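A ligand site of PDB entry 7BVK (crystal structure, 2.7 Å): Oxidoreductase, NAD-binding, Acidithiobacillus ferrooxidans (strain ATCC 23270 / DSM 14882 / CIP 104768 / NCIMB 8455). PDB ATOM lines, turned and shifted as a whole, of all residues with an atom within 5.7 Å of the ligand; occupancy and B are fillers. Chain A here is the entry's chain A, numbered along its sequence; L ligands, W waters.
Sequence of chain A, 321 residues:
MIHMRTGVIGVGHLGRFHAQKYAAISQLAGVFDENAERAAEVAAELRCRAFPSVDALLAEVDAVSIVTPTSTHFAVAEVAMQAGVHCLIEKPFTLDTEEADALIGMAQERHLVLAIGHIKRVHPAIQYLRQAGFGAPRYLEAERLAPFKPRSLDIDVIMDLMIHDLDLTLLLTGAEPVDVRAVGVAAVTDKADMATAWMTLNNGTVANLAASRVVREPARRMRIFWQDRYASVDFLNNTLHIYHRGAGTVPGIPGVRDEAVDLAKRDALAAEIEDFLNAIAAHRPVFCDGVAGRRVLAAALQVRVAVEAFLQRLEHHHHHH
Water W1 lies within hydrogen-bond range of an oxygen (O9) of the ligand (2.5 Å), the backbone carbonyl oxygen (O) of Val 67 (2.8 Å), the backbone NH (N) of Gly 12 (2.9 Å) and the backbone NH (N) of Gly 15 (3.3 Å).
The guanidinium group (NE) of Arg 38 is in hydrogen-bond range of an oxygen (O5) of the ligand, at 3.2 Å. The backbone carbonyl oxygen of Lys 91 sits at hydrogen-bond distance from an oxygen (O12) of the ligand, 3.4 Å away. An oxygen (O5) of the ligand is in hydrogen-bond range of the side-chain carboxylate of Asp 33, 2.5 Å away. The side-chain hydroxyl of Thr 70 lies within hydrogen-bond range of an oxygen (O12) of the ligand (3.4 Å). N of His 13 is in hydrogen-bond range of O2 of the ligand (3.5 Å). N of Glu 34 is in hydrogen-bond range of N5 of the ligand (3.4 Å).
Ile 9 touches the ligand. CA of Gly 10 touches N5 of the ligand, at 3.8 Å. CA of Gly 12 touches O2 of the ligand (3.6 Å). CD2 of Leu 14 touches O11 of the ligand, at 3.6 Å. Phe 32 touches the ligand. Asn 35 touches the ligand. O of Val 67 touches C11 of the ligand (3.4 Å). Thr 68 touches the ligand (CG2 to C10, 3.6 Å). CD of Pro 69 touches C6 of the ligand, 3.1 Å away. His 73 touches the ligand. Pro 92 touches the ligand. 17 residues have an atom within 4 Å of the ligand: Ile 9, Gly 10, Gly 12, His 13, Leu 14, Phe 32, Asp 33, Glu 34, Asn 35, Arg 38, Val 67, Thr 68, Pro 69, Thr 70, His 73, Lys 91 and Pro 92.
The backbone carbonyl oxygen of Pro 69 sits at hydrogen-bond distance from the side-chain hydroxyl of Thr 72, 2.5 Å away. The backbone NH (N) of Val 11 lies within hydrogen-bond range of the side-chain carboxylate (OD1) of Asp 33 (3.1 Å). The backbone carbonyl oxygen (O) of Phe 32 lies within hydrogen-bond range of the backbone NH (N) of Gly 10 (2.8 Å). The backbone NH (N) of Arg 38 lies within hydrogen-bond range of the side-chain amide oxygen (OD1) of Asn 35, at 3.0 Å. N of Val 67 is in hydrogen-bond range of O of Ile 9, 3.1 Å away. NE2 of His 73 sits at hydrogen-bond distance from O of Thr 68 (2.7 Å). OD2 of Asp 33 lies within hydrogen-bond range of N of Asn 35 (2.6 Å). NZ of Lys 91 lies within hydrogen-bond range of O of Asp 160 (3.1 Å).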
ATOM      1  N   ILE A   9      -0.664 -13.910  28.522  1.00  0.00           N
ATOM      2  CA  ILE A   9       0.622 -13.409  28.065  1.00  0.00           C
ATOM      3  C   ILE A   9       0.346 -12.392  26.961  1.00  0.00           C
ATOM      4  O   ILE A   9      -0.194 -12.728  25.896  1.00  0.00           O
ATOM      5  CB  ILE A   9       1.559 -14.539  27.600  1.00  0.00           C
ATOM      6  CG1 ILE A   9       1.627 -15.637  28.650  1.00  0.00           C
ATOM      7  CG2 ILE A   9       2.979 -13.998  27.362  1.00  0.00           C
ATOM      8  CD1 ILE A   9       2.252 -16.893  28.127  1.00  0.00           C
ATOM      9  N   GLY A  10       0.694 -11.145  27.235  1.00  0.00           N
ATOM     10  CA  GLY A  10       0.337 -10.047  26.376  1.00  0.00           C
ATOM     11  C   GLY A  10      -0.908  -9.383  26.909  1.00  0.00           C
ATOM     12  O   GLY A  10      -2.009  -9.902  26.701  1.00  0.00           O
ATOM     13  N   VAL A  11      -0.780  -8.258  27.604  1.00  0.00           N
ATOM     14  CA  VAL A  11      -2.004  -7.601  28.019  1.00  0.00           C
ATOM     15  C   VAL A  11      -2.015  -6.188  27.474  1.00  0.00           C
ATOM     16  O   VAL A  11      -1.927  -5.217  28.228  1.00  0.00           O
ATOM     17  CB  VAL A  11      -2.140  -7.622  29.556  1.00  0.00           C
ATOM     18  CG1 VAL A  11      -2.518  -9.034  30.036  1.00  0.00           C
ATOM     19  CG2 VAL A  11      -0.860  -7.148  30.253  1.00  0.00           C
ATOM     20  N   GLY A  12      -2.309  -6.084  26.189  1.00  0.00           N
ATOM     21  CA  GLY A  12      -2.596  -4.843  25.512  1.00  0.00           C
ATOM     22  C   GLY A  12      -4.088  -4.615  25.423  1.00  0.00           C
ATOM     23  O   GLY A  12      -4.855  -5.035  26.306  1.00  0.00           O
ATOM     24  N   HIS A  13      -4.522  -3.968  24.334  1.00  0.00           N
ATOM     25  CA  HIS A  13      -5.933  -3.641  24.179  1.00  0.00           C
ATOM     26  C   HIS A  13      -6.822  -4.875  24.342  1.00  0.00           C
ATOM     27  O   HIS A  13      -7.850  -4.814  25.022  1.00  0.00           O
ATOM     28  CB  HIS A  13      -6.178  -2.954  22.831  1.00  0.00           C
ATOM     29  CG  HIS A  13      -7.636  -2.721  22.530  1.00  0.00           C
ATOM     30  ND1 HIS A  13      -8.269  -3.255  21.422  1.00  0.00           N
ATOM     31  CD2 HIS A  13      -8.586  -2.027  23.204  1.00  0.00           C
ATOM     32  CE1 HIS A  13      -9.541  -2.898  21.430  1.00  0.00           C
ATOM     33  NE2 HIS A  13      -9.761  -2.147  22.499  1.00  0.00           N
ATOM     34  N   LEU A  14      -6.434  -6.013  23.770  1.00  0.00           N
ATOM     35  CA  LEU A  14      -7.246  -7.223  23.809  1.00  0.00           C
ATOM     36  C   LEU A  14      -6.873  -8.206  24.943  1.00  0.00           C
ATOM     37  O   LEU A  14      -7.755  -8.845  25.553  1.00  0.00           O
ATOM     38  CB  LEU A  14      -7.160  -7.911  22.451  1.00  0.00           C
ATOM     39  CG  LEU A  14      -8.192  -8.983  22.069  1.00  0.00           C
ATOM     40  CD1 LEU A  14      -9.636  -8.510  22.308  1.00  0.00           C
ATOM     41  CD2 LEU A  14      -7.959  -9.391  20.614  1.00  0.00           C
ATOM     42  N   GLY A  15      -5.573  -8.344  25.257  1.00  0.00           N
ATOM     43  CA  GLY A  15      -5.189  -9.226  26.349  1.00  0.00           C
ATOM     44  C   GLY A  15      -5.646  -8.742  27.708  1.00  0.00           C
ATOM     45  O   GLY A  15      -5.906  -9.550  28.598  1.00  0.00           O
ATOM     46  N   PHE A  32       1.821 -11.672  32.062  1.00  0.00           N
ATOM     47  CA  PHE A  32       3.157 -11.249  31.673  1.00  0.00           C
ATOM     48  C   PHE A  32       3.113 -10.431  30.385  1.00  0.00           C
ATOM     49  O   PHE A  32       2.356 -10.737  29.468  1.00  0.00           O
ATOM     50  CB  PHE A  32       4.125 -12.425  31.474  1.00  0.00           C
ATOM     51  CG  PHE A  32       5.456 -11.983  30.930  1.00  0.00           C
ATOM     52  CD1 PHE A  32       6.404 -11.424  31.786  1.00  0.00           C
ATOM     53  CD2 PHE A  32       5.731 -12.029  29.564  1.00  0.00           C
ATOM     54  CE1 PHE A  32       7.608 -10.972  31.296  1.00  0.00           C
ATOM     55  CE2 PHE A  32       6.942 -11.570  29.072  1.00  0.00           C
ATOM     56  CZ  PHE A  32       7.891 -11.050  29.940  1.00  0.00           C
ATOM     57  N   ASP A  33       3.979  -9.406  30.328  1.00  0.00           N
ATOM     58  CA  ASP A  33       4.109  -8.552  29.154  1.00  0.00           C
ATOM     59  C   ASP A  33       5.528  -7.980  29.077  1.00  0.00           C
ATOM     60  O   ASP A  33       6.151  -7.680  30.098  1.00  0.00           O
ATOM     61  CB  ASP A  33       3.076  -7.420  29.184  1.00  0.00           C
ATOM     62  CG  ASP A  33       2.970  -6.682  27.865  1.00  0.00           C
ATOM     63  OD1 ASP A  33       1.880  -6.723  27.250  1.00  0.00           O
ATOM     64  OD2 ASP A  33       3.970  -6.092  27.422  1.00  0.00           O
ATOM     65  N   GLU A  34       6.033  -7.797  27.843  1.00  0.00           N
ATOM     66  CA  GLU A  34       7.355  -7.203  27.653  1.00  0.00           C
ATOM     67  C   GLU A  34       7.379  -5.745  28.103  1.00  0.00           C
ATOM     68  O   GLU A  34       8.391  -5.273  28.650  1.00  0.00           O
ATOM     69  CB  GLU A  34       7.801  -7.320  26.183  1.00  0.00           C
ATOM     70  CG  GLU A  34       8.205  -8.735  25.707  1.00  0.00           C
ATOM     71  CD  GLU A  34       9.399  -9.372  26.477  1.00  0.00           C
ATOM     72  OE1 GLU A  34      10.544  -9.338  25.969  1.00  0.00           O
ATOM     73  OE2 GLU A  34       9.164  -9.928  27.574  1.00  0.00           O
ATOM     74  N   ASN A  35       6.287  -5.018  27.880  1.00  0.00           N
ATOM     75  CA  ASN A  35       6.061  -3.739  28.556  1.00  0.00           C
ATOM     76  C   ASN A  35       5.694  -3.995  30.023  1.00  0.00           C
ATOM     77  O   ASN A  35       4.688  -4.632  30.318  1.00  0.00           O
ATOM     78  CB  ASN A  35       4.976  -2.958  27.839  1.00  0.00           C
ATOM     79  CG  ASN A  35       4.871  -1.526  28.311  1.00  0.00           C
ATOM     80  OD1 ASN A  35       4.695  -1.256  29.496  1.00  0.00           O
ATOM     81  ND2 ASN A  35       4.965  -0.585  27.364  1.00  0.00           N
ATOM     82  N   ARG A  38       2.691  -1.606  31.714  1.00  0.00           N
ATOM     83  CA  ARG A  38       1.350  -2.017  31.266  1.00  0.00           C
ATOM     84  C   ARG A  38       0.883  -3.260  32.023  1.00  0.00           C
ATOM     85  O   ARG A  38      -0.271  -3.314  32.493  1.00  0.00           O
ATOM     86  CB  ARG A  38       1.374  -2.265  29.754  1.00  0.00           C
ATOM     87  CG  ARG A  38       0.184  -2.979  29.212  1.00  0.00           C
ATOM     88  CD  ARG A  38      -0.199  -2.525  27.803  1.00  0.00           C
ATOM     89  NE  ARG A  38       0.964  -2.309  26.946  1.00  0.00           N
ATOM     90  CZ  ARG A  38       1.327  -1.131  26.445  1.00  0.00           C
ATOM     91  NH1 ARG A  38       0.612  -0.042  26.743  1.00  0.00           N
ATOM     92  NH2 ARG A  38       2.401  -1.045  25.663  1.00  0.00           N
ATOM     93  N   VAL A  54       8.041 -14.858  31.304  1.00  0.00           N
ATOM     94  CA  VAL A  54       7.115 -15.864  30.792  1.00  0.00           C
ATOM     95  C   VAL A  54       7.120 -17.102  31.682  1.00  0.00           C
ATOM     96  O   VAL A  54       6.064 -17.668  32.008  1.00  0.00           O
ATOM     97  CB  VAL A  54       7.467 -16.242  29.336  1.00  0.00           C
ATOM     98  CG1 VAL A  54       6.247 -16.855  28.644  1.00  0.00           C
ATOM     99  CG2 VAL A  54       7.993 -15.047  28.563  1.00  0.00           C
ATOM    100  N   VAL A  67      -1.973 -13.442  23.491  1.00  0.00           N
ATOM    101  CA  VAL A  67      -2.549 -12.281  22.830  1.00  0.00           C
ATOM    102  C   VAL A  67      -1.392 -11.341  22.505  1.00  0.00           C
ATOM    103  O   VAL A  67      -1.524 -10.113  22.583  1.00  0.00           O
ATOM    104  CB  VAL A  67      -3.627 -11.607  23.702  1.00  0.00           C
ATOM    105  CG1 VAL A  67      -4.508 -10.717  22.874  1.00  0.00           C
ATOM    106  CG2 VAL A  67      -4.461 -12.647  24.424  1.00  0.00           C
ATOM    107  N   THR A  68      -0.234 -11.913  22.199  1.00  0.00           N
ATOM    108  CA  THR A  68       0.921 -11.139  21.764  1.00  0.00           C
ATOM    109  C   THR A  68       0.801 -10.864  20.268  1.00  0.00           C
ATOM    110  O   THR A  68      -0.027 -11.458  19.582  1.00  0.00           O
ATOM    111  CB  THR A  68       2.198 -11.888  22.128  1.00  0.00           C
ATOM    112  OG1 THR A  68       2.134 -13.224  21.602  1.00  0.00           O
ATOM    113  CG2 THR A  68       2.362 -11.926  23.650  1.00  0.00           C
ATOM    114  N   PRO A  69       1.595  -9.932  19.731  1.00  0.00           N
ATOM    115  CA  PRO A  69       1.508  -9.637  18.294  1.00  0.00           C
ATOM    116  C   PRO A  69       1.653 -10.905  17.477  1.00  0.00           C
ATOM    117  O   PRO A  69       2.345 -11.843  17.883  1.00  0.00           O
ATOM    118  CB  PRO A  69       2.674  -8.674  18.058  1.00  0.00           C
ATOM    119  CG  PRO A  69       2.867  -7.985  19.396  1.00  0.00           C
ATOM    120  CD  PRO A  69       2.540  -9.032  20.425  1.00  0.00           C
ATOM    121  N   THR A  70       0.990 -10.932  16.325  1.00  0.00           N
ATOM    122  CA  THR A  70       0.848 -12.175  15.580  1.00  0.00           C
ATOM    123  C   THR A  70       2.191 -12.814  15.250  1.00  0.00           C
ATOM    124  O   THR A  70       2.356 -14.025  15.381  1.00  0.00           O
ATOM    125  CB  THR A  70       0.070 -11.933  14.287  1.00  0.00           C
ATOM    126  OG1 THR A  70      -0.970 -10.984  14.533  1.00  0.00           O
ATOM    127  CG2 THR A  70      -0.532 -13.250  13.794  1.00  0.00           C
ATOM    128  N   THR A  72       4.634 -13.198  16.812  1.00  0.00           N
ATOM    129  CA  THR A  72       5.239 -13.835  17.973  1.00  0.00           C
ATOM    130  C   THR A  72       4.485 -15.071  18.442  1.00  0.00           C
ATOM    131  O   THR A  72       4.981 -15.776  19.332  1.00  0.00           O
ATOM    132  CB  THR A  72       5.334 -12.821  19.136  1.00  0.00           C
ATOM    133  OG1 THR A  72       4.013 -12.516  19.617  1.00  0.00           O
ATOM    134  CG2 THR A  72       5.961 -11.526  18.661  1.00  0.00           C
ATOM    135  N   HIS A  73       3.325 -15.363  17.852  1.00  0.00           N
ATOM    136  CA  HIS A  73       2.461 -16.407  18.405  1.00  0.00           C
ATOM    137  C   HIS A  73       3.168 -17.745  18.493  1.00  0.00           C
ATOM    138  O   HIS A  73       3.043 -18.453  19.493  1.00  0.00           O
ATOM    139  CB  HIS A  73       1.181 -16.562  17.575  1.00  0.00           C
ATOM    140  CG  HIS A  73       0.214 -15.429  17.736  1.00  0.00           C
ATOM    141  ND1 HIS A  73      -0.983 -15.379  17.059  1.00  0.00           N
ATOM    142  CD2 HIS A  73       0.279 -14.299  18.477  1.00  0.00           C
ATOM    143  CE1 HIS A  73      -1.614 -14.265  17.368  1.00  0.00           C
ATOM    144  NE2 HIS A  73      -0.875 -13.596  18.227  1.00  0.00           N
ATOM    145  N   VAL A  76       6.044 -17.652  21.578  1.00  0.00           N
ATOM    146  CA  VAL A  76       5.419 -17.766  22.891  1.00  0.00           C
ATOM    147  C   VAL A  76       4.754 -19.126  23.047  1.00  0.00           C
ATOM    148  O   VAL A  76       4.923 -19.802  24.076  1.00  0.00           O
ATOM    149  CB  VAL A  76       4.443 -16.611  23.128  1.00  0.00           C
ATOM    150  CG1 VAL A  76       3.809 -16.761  24.513  1.00  0.00           C
ATOM    151  CG2 VAL A  76       5.162 -15.296  22.984  1.00  0.00           C
ATOM    152  N   GLU A  90      -5.042 -15.927  20.265  1.00  0.00           N
ATOM    153  CA  GLU A  90      -5.922 -14.939  19.591  1.00  0.00           C
ATOM    154  C   GLU A  90      -5.681 -14.964  18.079  1.00  0.00           C
ATOM    155  O   GLU A  90      -4.522 -15.217  17.678  1.00  0.00           O
ATOM    156  CB  GLU A  90      -5.700 -13.537  20.163  1.00  0.00           C
ATOM    157  CG  GLU A  90      -6.835 -13.057  21.055  1.00  0.00           C
ATOM    158  CD  GLU A  90      -8.115 -12.713  20.309  1.00  0.00           C
ATOM    159  OE1 GLU A  90      -9.196 -12.908  20.889  1.00  0.00           O
ATOM    160  OE2 GLU A  90      -8.018 -12.246  19.158  1.00  0.00           O
ATOM    161  N   LYS A  91      -6.706 -14.672  17.264  1.00  0.00           N
ATOM    162  CA  LYS A  91      -6.535 -14.704  15.787  1.00  0.00           C
ATOM    163  C   LYS A  91      -5.656 -13.541  15.284  1.00  0.00           C
ATOM    164  O   LYS A  91      -5.665 -12.491  15.890  1.00  0.00           O
ATOM    165  CB  LYS A  91      -7.836 -14.904  15.010  1.00  0.00           C
ATOM    166  CG  LYS A  91      -8.794 -13.718  14.952  1.00  0.00           C
ATOM    167  CD  LYS A  91      -8.639 -12.849  13.765  1.00  0.00           C
ATOM    168  CE  LYS A  91      -8.730 -11.378  14.113  1.00  0.00           C
ATOM    169  NZ  LYS A  91      -9.819 -10.686  13.373  1.00  0.00           N
ATOM    170  N   PRO A  92      -4.902 -13.684  14.181  1.00  0.00           N
ATOM    171  CA  PRO A  92      -4.800 -14.927  13.402  1.00  0.00           C
ATOM    172  C   PRO A  92      -3.900 -15.943  14.091  1.00  0.00           C
ATOM    173  O   PRO A  92      -3.168 -15.543  14.927  1.00  0.00           O
ATOM    174  CB  PRO A  92      -4.101 -14.521  12.110  1.00  0.00           C
ATOM    175  CG  PRO A  92      -4.046 -13.029  12.147  1.00  0.00           C
ATOM    176  CD  PRO A  92      -4.118 -12.632  13.598  1.00  0.00           C
ATOM    177  N   ASP A 160      -7.047  -9.952   8.424  1.00  0.00           N
ATOM    178  CA  ASP A 160      -7.716  -9.318   9.536  1.00  0.00           C
ATOM    179  C   ASP A 160      -9.232  -9.460   9.456  1.00  0.00           C
ATOM    180  O   ASP A 160      -9.846 -10.013  10.368  1.00  0.00           O
ATOM    181  CB  ASP A 160      -7.344  -7.846   9.595  1.00  0.00           C
ATOM    182  CG  ASP A 160      -8.093  -7.103  10.683  1.00  0.00           C
ATOM    183  OD1 ASP A 160      -8.942  -6.271  10.281  1.00  0.00           O
ATOM    184  OD2 ASP A 160      -7.855  -7.338  11.893  1.00  0.00           O
HETATM  185  P1  LIG L   1      -1.453  -4.831  21.285  1.00  0.00           P
HETATM  186  O1  LIG L   1      -0.420  -4.927  20.289  1.00  0.00           O
HETATM  187  O2  LIG L   1      -1.853  -3.755  22.124  1.00  0.00           O
HETATM  188  O3  LIG L   1      -0.990  -5.983  22.343  1.00  0.00           O
HETATM  189  C1  LIG L   1       0.392  -6.102  22.453  1.00  0.00           C
HETATM  190  C2  LIG L   1       0.879  -6.509  23.790  1.00  0.00           C
HETATM  191  O4  LIG L   1       1.745  -7.510  23.614  1.00  0.00           O
HETATM  192  C3  LIG L   1       1.657  -5.317  24.159  1.00  0.00           C
HETATM  193  O5  LIG L   1       1.335  -5.116  25.403  1.00  0.00           O
HETATM  194  C4  LIG L   1       3.071  -5.740  23.943  1.00  0.00           C
HETATM  195  O6  LIG L   1       3.904  -5.171  24.845  1.00  0.00           O
HETATM  196  C5  LIG L   1       2.898  -7.177  24.258  1.00  0.00           C
HETATM  197  N1  LIG L   1       3.915  -8.060  23.784  1.00  0.00           N
HETATM  198  C6  LIG L   1       4.540  -8.104  22.662  1.00  0.00           C
HETATM  199  N2  LIG L   1       5.341  -9.077  22.591  1.00  0.00           N
HETATM  200  C7  LIG L   1       5.223  -9.679  23.705  1.00  0.00           C
HETATM  201  C8  LIG L   1       5.798 -10.780  24.220  1.00  0.00           C
HETATM  202  N3  LIG L   1       6.656 -11.360  23.469  1.00  0.00           N
HETATM  203  N4  LIG L   1       5.532 -11.258  25.413  1.00  0.00           N
HETATM  204  C9  LIG L   1       4.631 -10.593  26.093  1.00  0.00           C
HETATM  205  N5  LIG L   1       4.011  -9.530  25.711  1.00  0.00           N
HETATM  206  C10 LIG L   1       4.343  -9.092  24.499  1.00  0.00           C
HETATM  207  O7  LIG L   1      -2.488  -5.218  20.251  1.00  0.00           O
HETATM  208  P2  LIG L   1      -3.521  -6.285  20.426  1.00  0.00           P
HETATM  209  O8  LIG L   1      -4.743  -6.193  19.603  1.00  0.00           O
HETATM  210  O9  LIG L   1      -3.363  -6.722  21.772  1.00  0.00           O
HETATM  211  O10 LIG L   1      -2.798  -7.541  19.646  1.00  0.00           O
HETATM  212  C11 LIG L   1      -3.287  -8.687  20.030  1.00  0.00           C
HETATM  213  C12 LIG L   1      -4.034  -9.349  18.901  1.00  0.00           C
HETATM  214  O11 LIG L   1      -5.125  -8.505  18.573  1.00  0.00           O
HETATM  215  C13 LIG L   1      -3.151  -9.420  17.628  1.00  0.00           C
HETATM  216  O12 LIG L   1      -3.075 -10.765  17.241  1.00  0.00           O
HETATM  217  C14 LIG L   1      -4.006  -8.601  16.673  1.00  0.00           C
HETATM  218  O13 LIG L   1      -4.166  -9.161  15.463  1.00  0.00           O
HETATM  219  C15 LIG L   1      -5.383  -8.694  17.315  1.00  0.00           C
HETATM  220  O   HOH W   1      -2.596  -7.834  23.874  1.00  0.00           O
